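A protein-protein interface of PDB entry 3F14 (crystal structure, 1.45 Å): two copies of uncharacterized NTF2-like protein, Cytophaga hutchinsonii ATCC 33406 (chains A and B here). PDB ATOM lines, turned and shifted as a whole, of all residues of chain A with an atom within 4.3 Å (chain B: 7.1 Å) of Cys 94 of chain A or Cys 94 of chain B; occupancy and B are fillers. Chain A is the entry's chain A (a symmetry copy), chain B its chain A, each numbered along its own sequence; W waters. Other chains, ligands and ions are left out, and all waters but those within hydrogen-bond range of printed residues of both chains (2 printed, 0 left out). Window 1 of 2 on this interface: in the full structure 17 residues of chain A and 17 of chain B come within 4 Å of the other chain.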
ATOM      1  N   VAL A  74     -20.329  19.767  -4.601  1.00  0.00           N
ATOM      2  CA  VAL A  74     -21.448  18.869  -4.334  1.00  0.00           C
ATOM      3  C   VAL A  74     -22.314  19.502  -3.252  1.00  0.00           C
ATOM      4  O   VAL A  74     -21.765  19.894  -2.209  1.00  0.00           O
ATOM      5  CB  VAL A  74     -20.944  17.485  -3.882  1.00  0.00           C
ATOM      6  CG1 VAL A  74     -22.123  16.548  -3.584  1.00  0.00           C
ATOM      7  CG2 VAL A  74     -19.953  16.865  -4.929  1.00  0.00           C
ATOM      8  N   ILE A  75     -23.595  19.651  -3.505  1.00  0.00           N
ATOM      9  CA  ILE A  75     -24.556  20.184  -2.534  1.00  0.00           C
ATOM     10  C   ILE A  75     -25.605  19.128  -2.267  1.00  0.00           C
ATOM     11  O   ILE A  75     -26.200  18.589  -3.206  1.00  0.00           O
ATOM     12  CB  ILE A  75     -25.236  21.453  -3.019  1.00  0.00           C
ATOM     13  CG1 ILE A  75     -24.138  22.510  -3.309  1.00  0.00           C
ATOM     14  CG2 ILE A  75     -26.368  21.912  -2.020  1.00  0.00           C
ATOM     15  CD1 ILE A  75     -24.598  23.977  -3.472  1.00  0.00           C
ATOM     16  N   TYR A  93     -31.998  15.600  -2.331  1.00  0.00           N
ATOM     17  CA  TYR A  93     -31.162  15.751  -3.514  1.00  0.00           C
ATOM     18  C   TYR A  93     -29.682  15.899  -3.224  1.00  0.00           C
ATOM     19  O   TYR A  93     -29.259  16.401  -2.190  1.00  0.00           O
ATOM     20  CB  TYR A  93     -31.642  16.949  -4.415  1.00  0.00           C
ATOM     21  CG  TYR A  93     -31.683  18.296  -3.745  1.00  0.00           C
ATOM     22  CD1 TYR A  93     -30.535  19.095  -3.587  1.00  0.00           C
ATOM     23  CD2 TYR A  93     -32.887  18.817  -3.299  1.00  0.00           C
ATOM     24  CE1 TYR A  93     -30.606  20.324  -2.960  1.00  0.00           C
ATOM     25  CE2 TYR A  93     -32.965  20.068  -2.732  1.00  0.00           C
ATOM     26  CZ  TYR A  93     -31.839  20.825  -2.545  1.00  0.00           C
ATOM     27  OH  TYR A  93     -31.970  22.062  -1.917  1.00  0.00           O
ATOM     28  N   CYS A  94     -28.908  15.426  -4.184  1.00  0.00           N
ATOM     29  CA  CYS A  94     -27.478  15.632  -4.223  1.00  0.00           C
ATOM     30  C   CYS A  94     -27.159  16.141  -5.642  1.00  0.00           C
ATOM     31  O   CYS A  94     -27.361  15.424  -6.610  1.00  0.00           O
ATOM     32  CB  CYS A  94     -26.728  14.334  -3.923  1.00  0.00           C
ATOM     33  SG  CYS A  94     -24.925  14.548  -4.040  1.00  0.00           S
ATOM     34  N   ASP A  95     -26.673  17.380  -5.722  1.00  0.00           N
ATOM     35  CA  ASP A  95     -26.322  18.050  -6.977  1.00  0.00           C
ATOM     36  C   ASP A  95     -24.826  18.187  -7.066  1.00  0.00           C
ATOM     37  O   ASP A  95     -24.180  18.742  -6.172  1.00  0.00           O
ATOM     38  CB  ASP A  95     -26.962  19.425  -7.072  1.00  0.00           C
ATOM     39  CG  ASP A  95     -28.479  19.393  -7.060  1.00  0.00           C
ATOM     40  OD1 ASP A  95     -29.104  18.476  -7.626  1.00  0.00           O
ATOM     41  OD2 ASP A  95     -29.115  20.356  -6.466  1.00  0.00           O
ATOM     42  N   ILE A  96     -24.258  17.726  -8.185  1.00  0.00           N
ATOM     43  CA  ILE A  96     -22.813  17.730  -8.411  1.00  0.00           C
ATOM     44  C   ILE A  96     -22.498  18.641  -9.602  1.00  0.00           C
ATOM     45  O   ILE A  96     -23.039  18.433 -10.700  1.00  0.00           O
ATOM     46  CB  ILE A  96     -22.294  16.304  -8.714  1.00  0.00           C
ATOM     47  CG1 ILE A  96     -22.653  15.365  -7.584  1.00  0.00           C
ATOM     48  CG2 ILE A  96     -20.780  16.318  -9.009  1.00  0.00           C
ATOM     49  CD1 ILE A  96     -22.281  13.874  -7.829  1.00  0.00           C
ATOM     50  N   THR A 108     -25.034  17.170 -12.296  1.00  0.00           N
ATOM     51  CA  THR A 108     -25.583  15.817 -12.146  1.00  0.00           C
ATOM     52  C   THR A 108     -26.438  15.796 -10.885  1.00  0.00           C
ATOM     53  O   THR A 108     -25.919  16.142  -9.814  1.00  0.00           O
ATOM     54  CB  THR A 108     -24.459  14.785 -12.052  1.00  0.00           C
ATOM     55  OG1 THR A 108     -23.562  14.911 -13.173  1.00  0.00           O
ATOM     56  CG2 THR A 108     -25.057  13.343 -12.036  1.00  0.00           C
ATOM     57  N   SER A 109     -27.718  15.450 -10.992  1.00  0.00           N
ATOM     58  CA  SER A 109     -28.605  15.503  -9.819  1.00  0.00           C
ATOM     59  C   SER A 109     -29.185  14.129  -9.512  1.00  0.00           C
ATOM     60  O   SER A 109     -29.798  13.491 -10.372  1.00  0.00           O
ATOM     61  CB  SER A 109     -29.725  16.485 -10.054  1.00  0.00           C
ATOM     62  OG  SER A 109     -29.274  17.830 -10.250  1.00  0.00           O
ATOM     63  N   TYR A 110     -28.996  13.716  -8.255  1.00  0.00           N
ATOM     64  CA  TYR A 110     -29.620  12.512  -7.685  1.00  0.00           C
ATOM     65  C   TYR A 110     -30.745  12.972  -6.805  1.00  0.00           C
ATOM     66  O   TYR A 110     -30.508  13.628  -5.799  1.00  0.00           O
ATOM     67  CB  TYR A 110     -28.595  11.721  -6.851  1.00  0.00           C
ATOM     68  CG  TYR A 110     -27.420  11.212  -7.625  1.00  0.00           C
ATOM     69  CD1 TYR A 110     -26.377  12.040  -8.032  1.00  0.00           C
ATOM     70  CD2 TYR A 110     -27.286   9.847  -7.899  1.00  0.00           C
ATOM     71  CE1 TYR A 110     -25.292  11.541  -8.781  1.00  0.00           C
ATOM     72  CE2 TYR A 110     -26.245   9.366  -8.628  1.00  0.00           C
ATOM     73  CZ  TYR A 110     -25.195  10.204  -9.101  1.00  0.00           C
ATOM     74  OH  TYR A 110     -24.150   9.683  -9.820  1.00  0.00           O
ATOM     75  N   SER B  14     -17.522   1.743  -1.993  1.00  0.00           N
ATOM     76  CA  SER B  14     -18.485   2.049  -3.044  1.00  0.00           C
ATOM     77  C   SER B  14     -18.668   0.884  -4.024  1.00  0.00           C
ATOM     78  O   SER B  14     -19.724   0.698  -4.588  1.00  0.00           O
ATOM     79  CB  SER B  14     -18.101   3.334  -3.796  1.00  0.00           C
ATOM     80  OG  SER B  14     -18.507   4.501  -3.033  1.00  0.00           O
ATOM     81  N   ILE B  34     -30.161   7.190   1.849  1.00  0.00           N
ATOM     82  CA  ILE B  34     -31.198   8.176   1.621  1.00  0.00           C
ATOM     83  C   ILE B  34     -32.493   7.532   1.124  1.00  0.00           C
ATOM     84  O   ILE B  34     -32.504   6.742   0.195  1.00  0.00           O
ATOM     85  CB  ILE B  34     -30.701   9.226   0.570  1.00  0.00           C
ATOM     86  CG1 ILE B  34     -29.493  10.017   1.105  1.00  0.00           C
ATOM     87  CG2 ILE B  34     -31.832  10.169   0.160  1.00  0.00           C
ATOM     88  CD1 ILE B  34     -29.781  11.014   2.190  1.00  0.00           C
ATOM     89  N   VAL B  74     -16.551  12.021  -2.570  1.00  0.00           N
ATOM     90  CA  VAL B  74     -17.803  11.659  -3.225  1.00  0.00           C
ATOM     91  C   VAL B  74     -17.477  10.740  -4.397  1.00  0.00           C
ATOM     92  O   VAL B  74     -16.607  11.101  -5.207  1.00  0.00           O
ATOM     93  CB  VAL B  74     -18.546  12.917  -3.717  1.00  0.00           C
ATOM     94  CG1 VAL B  74     -19.855  12.533  -4.422  1.00  0.00           C
ATOM     95  CG2 VAL B  74     -18.788  13.934  -2.548  1.00  0.00           C
ATOM     96  N   ILE B  75     -18.096   9.583  -4.455  1.00  0.00           N
ATOM     97  CA  ILE B  75     -17.929   8.629  -5.556  1.00  0.00           C
ATOM     98  C   ILE B  75     -19.273   8.414  -6.215  1.00  0.00           C
ATOM     99  O   ILE B  75     -20.260   8.114  -5.535  1.00  0.00           O
ATOM    100  CB  ILE B  75     -17.381   7.289  -5.093  1.00  0.00           C
ATOM    101  CG1 ILE B  75     -16.016   7.540  -4.398  1.00  0.00           C
ATOM    102  CG2 ILE B  75     -17.356   6.243  -6.272  1.00  0.00           C
ATOM    103  CD1 ILE B  75     -15.109   6.309  -4.163  1.00  0.00           C
ATOM    104  N   GLU B  76     -19.335   8.604  -7.516  1.00  0.00           N
ATOM    105  CA  GLU B  76     -20.465   8.191  -8.341  1.00  0.00           C
ATOM    106  C   GLU B  76     -20.171   6.890  -8.999  1.00  0.00           C
ATOM    107  O   GLU B  76     -19.036   6.682  -9.440  1.00  0.00           O
ATOM    108  CB  GLU B  76     -20.711   9.220  -9.434  1.00  0.00           C
ATOM    109  CG  GLU B  76     -21.052  10.637  -8.922  1.00  0.00           C
ATOM    110  CD  GLU B  76     -21.359  11.568 -10.087  1.00  0.00           C
ATOM    111  OE1 GLU B  76     -22.459  11.436 -10.693  1.00  0.00           O
ATOM    112  OE2 GLU B  76     -20.487  12.409 -10.423  1.00  0.00           O
ATOM    113  N   GLY B  77     -21.166   6.058  -9.177  1.00  0.00           N
ATOM    114  CA  GLY B  77     -20.990   4.824  -9.910  1.00  0.00           C
ATOM    115  C   GLY B  77     -22.285   4.131 -10.234  1.00  0.00           C
ATOM    116  O   GLY B  77     -23.369   4.712 -10.019  1.00  0.00           O
ATOM    117  N   SER B  92     -27.915   3.622 -10.087  1.00  0.00           N
ATOM    118  CA  SER B  92     -26.940   4.670 -10.122  1.00  0.00           C
ATOM    119  C   SER B  92     -26.762   5.168  -8.694  1.00  0.00           C
ATOM    120  O   SER B  92     -27.767   5.489  -8.032  1.00  0.00           O
ATOM    121  CB  SER B  92     -27.427   5.823 -11.004  1.00  0.00           C
ATOM    122  OG  SER B  92     -27.463   5.433 -12.385  1.00  0.00           O
ATOM    123  N   TYR B  93     -25.530   5.229  -8.222  1.00  0.00           N
ATOM    124  CA  TYR B  93     -25.262   5.664  -6.859  1.00  0.00           C
ATOM    125  C   TYR B  93     -24.287   6.819  -6.747  1.00  0.00           C
ATOM    126  O   TYR B  93     -23.397   7.013  -7.566  1.00  0.00           O
ATOM    127  CB  TYR B  93     -24.769   4.473  -5.955  1.00  0.00           C
ATOM    128  CG  TYR B  93     -23.530   3.762  -6.429  1.00  0.00           C
ATOM    129  CD1 TYR B  93     -22.236   4.259  -6.187  1.00  0.00           C
ATOM    130  CD2 TYR B  93     -23.633   2.548  -7.090  1.00  0.00           C
ATOM    131  CE1 TYR B  93     -21.120   3.585  -6.643  1.00  0.00           C
ATOM    132  CE2 TYR B  93     -22.517   1.848  -7.487  1.00  0.00           C
ATOM    133  CZ  TYR B  93     -21.261   2.354  -7.283  1.00  0.00           C
ATOM    134  OH  TYR B  93     -20.169   1.627  -7.754  1.00  0.00           O
ATOM    135  N   CYS B  94     -24.501   7.589  -5.695  1.00  0.00           N
ATOM    136  CA  CYS B  94     -23.588   8.626  -5.273  1.00  0.00           C
ATOM    137  C   CYS B  94     -23.363   8.407  -3.764  1.00  0.00           C
ATOM    138  O   CYS B  94     -24.293   8.523  -2.981  1.00  0.00           O
ATOM    139  CB  CYS B  94     -24.170  10.013  -5.544  1.00  0.00           C
ATOM    140  SG  CYS B  94     -23.073  11.339  -4.952  1.00  0.00           S
ATOM    141  N   ASP B  95     -22.121   8.084  -3.400  1.00  0.00           N
ATOM    142  CA  ASP B  95     -21.705   7.821  -2.020  1.00  0.00           C
ATOM    143  C   ASP B  95     -20.826   8.945  -1.542  1.00  0.00           C
ATOM    144  O   ASP B  95     -19.811   9.272  -2.164  1.00  0.00           O
ATOM    145  CB  ASP B  95     -20.952   6.507  -1.907  1.00  0.00           C
ATOM    146  CG  ASP B  95     -21.776   5.296  -2.303  1.00  0.00           C
ATOM    147  OD1 ASP B  95     -22.993   5.235  -2.038  1.00  0.00           O
ATOM    148  OD2 ASP B  95     -21.184   4.310  -2.903  1.00  0.00           O
ATOM    149  N   ILE B  96     -21.180   9.519  -0.388  1.00  0.00           N
ATOM    150  CA  ILE B  96     -20.470  10.660   0.191  1.00  0.00           C
ATOM    151  C   ILE B  96     -19.862  10.238   1.534  1.00  0.00           C
ATOM    152  O   ILE B  96     -20.591   9.772   2.423  1.00  0.00           O
ATOM    153  CB  ILE B  96     -21.427  11.852   0.422  1.00  0.00           C
ATOM    154  CG1 ILE B  96     -22.096  12.246  -0.876  1.00  0.00           C
ATOM    155  CG2 ILE B  96     -20.690  13.033   1.085  1.00  0.00           C
ATOM    156  CD1 ILE B  96     -23.170  13.365  -0.747  1.00  0.00           C
ATOM    157  N   TYR B  97     -18.538  10.343   1.652  1.00  0.00           N
ATOM    158  CA  TYR B  97     -17.828   9.934   2.857  1.00  0.00           C
ATOM    159  C   TYR B  97     -17.310  11.128   3.590  1.00  0.00           C
ATOM    160  O   TYR B  97     -16.709  12.009   2.981  1.00  0.00           O
ATOM    161  CB  TYR B  97     -16.630   9.028   2.484  1.00  0.00           C
ATOM    162  CG  TYR B  97     -16.992   7.770   1.716  1.00  0.00           C
ATOM    163  CD1 TYR B  97     -17.219   7.810   0.341  1.00  0.00           C
ATOM    164  CD2 TYR B  97     -17.127   6.542   2.348  1.00  0.00           C
ATOM    165  CE1 TYR B  97     -17.599   6.713  -0.371  1.00  0.00           C
ATOM    166  CE2 TYR B  97     -17.502   5.437   1.653  1.00  0.00           C
ATOM    167  CZ  TYR B  97     -17.717   5.506   0.280  1.00  0.00           C
ATOM    168  OH  TYR B  97     -18.135   4.405  -0.410  1.00  0.00           O
ATOM    169  N   ILE B 107     -21.171   7.844   6.073  1.00  0.00           N
ATOM    170  CA  ILE B 107     -21.399   7.518   4.677  1.00  0.00           C
ATOM    171  C   ILE B 107     -22.845   7.916   4.377  1.00  0.00           C
ATOM    172  O   ILE B 107     -23.726   7.571   5.150  1.00  0.00           O
ATOM    173  CB  ILE B 107     -21.196   6.024   4.354  1.00  0.00           C
ATOM    174  CG1 ILE B 107     -19.866   5.534   4.942  1.00  0.00           C
ATOM    175  CG2 ILE B 107     -21.312   5.843   2.809  1.00  0.00           C
ATOM    176  CD1 ILE B 107     -19.640   4.031   4.772  1.00  0.00           C
ATOM    177  N   THR B 108     -23.070   8.661   3.286  1.00  0.00           N
ATOM    178  CA  THR B 108     -24.420   9.006   2.825  1.00  0.00           C
ATOM    179  C   THR B 108     -24.574   8.491   1.398  1.00  0.00           C
ATOM    180  O   THR B 108     -23.751   8.858   0.548  1.00  0.00           O
ATOM    181  CB  THR B 108     -24.640  10.518   2.880  1.00  0.00           C
ATOM    182  OG1 THR B 108     -24.344  11.025   4.195  1.00  0.00           O
ATOM    183  CG2 THR B 108     -26.121  10.856   2.523  1.00  0.00           C
ATOM    184  N   SER B 109     -25.558   7.635   1.135  1.00  0.00           N
ATOM    185  CA  SER B 109     -25.690   7.042  -0.205  1.00  0.00           C
ATOM    186  C   SER B 109     -27.034   7.396  -0.827  1.00  0.00           C
ATOM    187  O   SER B 109     -28.090   7.148  -0.240  1.00  0.00           O
ATOM    188  CB  SER B 109     -25.543   5.544  -0.130  1.00  0.00           C
ATOM    189  OG  SER B 109     -24.263   5.117   0.350  1.00  0.00           O
ATOM    190  N   TYR B 110     -26.954   7.951  -2.041  1.00  0.00           N
ATOM    191  CA  TYR B 110     -28.118   8.206  -2.902  1.00  0.00           C
ATOM    192  C   TYR B 110     -28.119   7.149  -3.967  1.00  0.00           C
ATOM    193  O   TYR B 110     -27.211   7.101  -4.785  1.00  0.00           O
ATOM    194  CB  TYR B 110     -28.010   9.599  -3.551  1.00  0.00           C
ATOM    195  CG  TYR B 110     -27.995  10.739  -2.582  1.00  0.00           C
ATOM    196  CD1 TYR B 110     -26.874  11.059  -1.821  1.00  0.00           C
ATOM    197  CD2 TYR B 110     -29.099  11.589  -2.467  1.00  0.00           C
ATOM    198  CE1 TYR B 110     -26.893  12.124  -0.897  1.00  0.00           C
ATOM    199  CE2 TYR B 110     -29.122  12.610  -1.572  1.00  0.00           C
ATOM    200  CZ  TYR B 110     -28.006  12.922  -0.744  1.00  0.00           C
ATOM    201  OH  TYR B 110     -28.056  13.971   0.138  1.00  0.00           O
ATOM    202  N   CYS B 111     -29.162   6.317  -4.016  1.00  0.00           N
ATOM    203  CA  CYS B 111     -29.217   5.160  -4.907  1.00  0.00           C
ATOM    204  C   CYS B 111     -30.515   5.215  -5.662  1.00  0.00           C
ATOM    205  O   CYS B 111     -31.584   5.244  -5.056  1.00  0.00           O
ATOM    206  CB  CYS B 111     -29.146   3.845  -4.116  1.00  0.00           C
ATOM    207  SG  CYS B 111     -27.741   3.697  -2.997  1.00  0.00           S
ATOM    208  N   ILE B 112     -30.424   5.240  -6.968  1.00  0.00           N
ATOM    209  CA  ILE B 112     -31.575   5.377  -7.873  1.00  0.00           C
ATOM    210  C   ILE B 112     -31.600   4.246  -8.874  1.00  0.00           C
ATOM    211  O   ILE B 112     -30.682   4.138  -9.685  1.00  0.00           O
ATOM    212  CB  ILE B 112     -31.544   6.756  -8.589  1.00  0.00           C
ATOM    213  CG1 ILE B 112     -31.681   7.853  -7.543  1.00  0.00           C
ATOM    214  CG2 ILE B 112     -32.664   6.907  -9.639  1.00  0.00           C
ATOM    215  CD1 ILE B 112     -31.445   9.289  -8.041  1.00  0.00           C
ATOM    216  OXT ILE B 112     -32.636   3.563  -8.945  1.00  0.00           O
HETATM  217  O   HOH W   1     -20.893  13.982 -12.441  1.00  0.00           O
HETATM  218  O   HOH W   2     -24.016   7.257 -11.067  1.00  0.00           O
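OE1 of Glu 76 of chain B sits at hydrogen-bond distance from OH of Tyr 110 of chain A (2.6 Å).
The backbone NH (N) of Ser 92 of chain B sits at hydrogen-bond distance from the chain-end carboxylate (O) of Ile 112 of chain B, 2.8 Å away.
The backbone NH (N) of Ile 96 of chain B lies within hydrogen-bond range of the backbone carbonyl oxygen (O) of Thr 108 of chain B (2.8 Å).
O of Gly 77 of chain B is in hydrogen-bond range of N of Tyr 93 of chain B (2.9 Å).
O of Cys 94 of chain B is in hydrogen-bond range of N of Tyr 110 of chain B, 2.9 Å away.
O of Cys 94 of chain A lies within hydrogen-bond range of N of Tyr 110 of chain A, 2.9 Å away.
N of Ile 96 of chain A lies within hydrogen-bond range of O of Thr 108 of chain A.
CG2 of Val 74 of chain A touches CG2 of Val 74 of chain B, 3.95 Å away.
OH of Tyr 110 of chain B touches O of Tyr 93 of chain A, at 3.6 Å.
Cys 94 of chain A touches Cys 94 of chain B (SG to SG, 3.8 Å).
CD1 of Ile 96 of chain B touches SG of Cys 94 of chain A, 3.9 Å away.
Cys 94 of chain A touches Tyr 110 of chain B (CB to CZ, 3.7 Å).
Ile 96 of chain A touches Glu 76 of chain B (CD1 to CD, 3.4 Å).
Ile 96 of chain A touches Cys 94 of chain B.
Thr 108 of chain A touches Glu 76 of chain B (CG2 to OE1, 3.5 Å).
Tyr 110 of chain A touches Tyr 110 of chain B (CB to CB, 3.97 Å).
Ile 112 of chain B touches Tyr 110 of chain A.
Of the printed residues of chain B, Val 74 of chain A touches Val 74.
Of the printed residues of chain B, Cys 94 of chain A touches Cys 94 (3.8 Å), Ile 96 (3.9 Å) and Tyr 110 (3.7 Å).
Of the printed residues of chain B, Thr 108 of chain A touches Glu 76.
Of the printed residues of chain A, Val 74 of chain B touches Val 74 (3.95 Å).
Of the printed residues of chain A, Ile 96 of chain B touches Cys 94.
Of the printed residues of chain A, Tyr 110 of chain B touches Tyr 93 (3.6 Å), Cys 94 (3.7 Å) and Tyr 110 (3.97 Å).
Cys 111 of chain B touches none of the printed residues of chain A.
The nearest residue of chain B that does not touch Cys 94 of chain A is Val 74 of chain B (5.5 Å).
Of the 18 printed residues of chain B, 7 touch a printed residue of chain A.
Hydrophobic or aromatic side chains of chain B within 4 Å of the printed part of chain A: Val 74, Ile 96, Tyr 110 and Ile 112.
Of the 9 printed residues of chain A, 6 touch a printed residue of chain B.
Tyr 93 of chain A touches Tyr 110 of chain B, and with the chains exchanged Tyr 110 of chain A touches Tyr 93 of chain B.
Cys 94 of chain A touches its own counterpart, Cys 94 of chain B.
Cys 94 of chain A touches Ile 96 of chain B, and with the chains exchanged Ile 96 of chain A touches Cys 94 of chain B.
Tyr 110 of chain A touches its own counterpart, Tyr 110 of chain B.
Positions printed for both chains: 74, 75, 93, 94, 95, 96, 108, 109 and 110.
Of the 13 pairs that touch across the chains among the printed residues, 9 have their exchanged pair printed and touching as well.
Water W1 lies within hydrogen-bond range of OE2 of Glu 76 of chain B and OG1 of Thr 108 of chain A.
Water W2 bridges the side-chain hydroxyl (OH) of Tyr 110 of chain A (2.7 Å) and the backbone carbonyl oxygen (O) of Gly 77 of chain B (2.8 Å).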
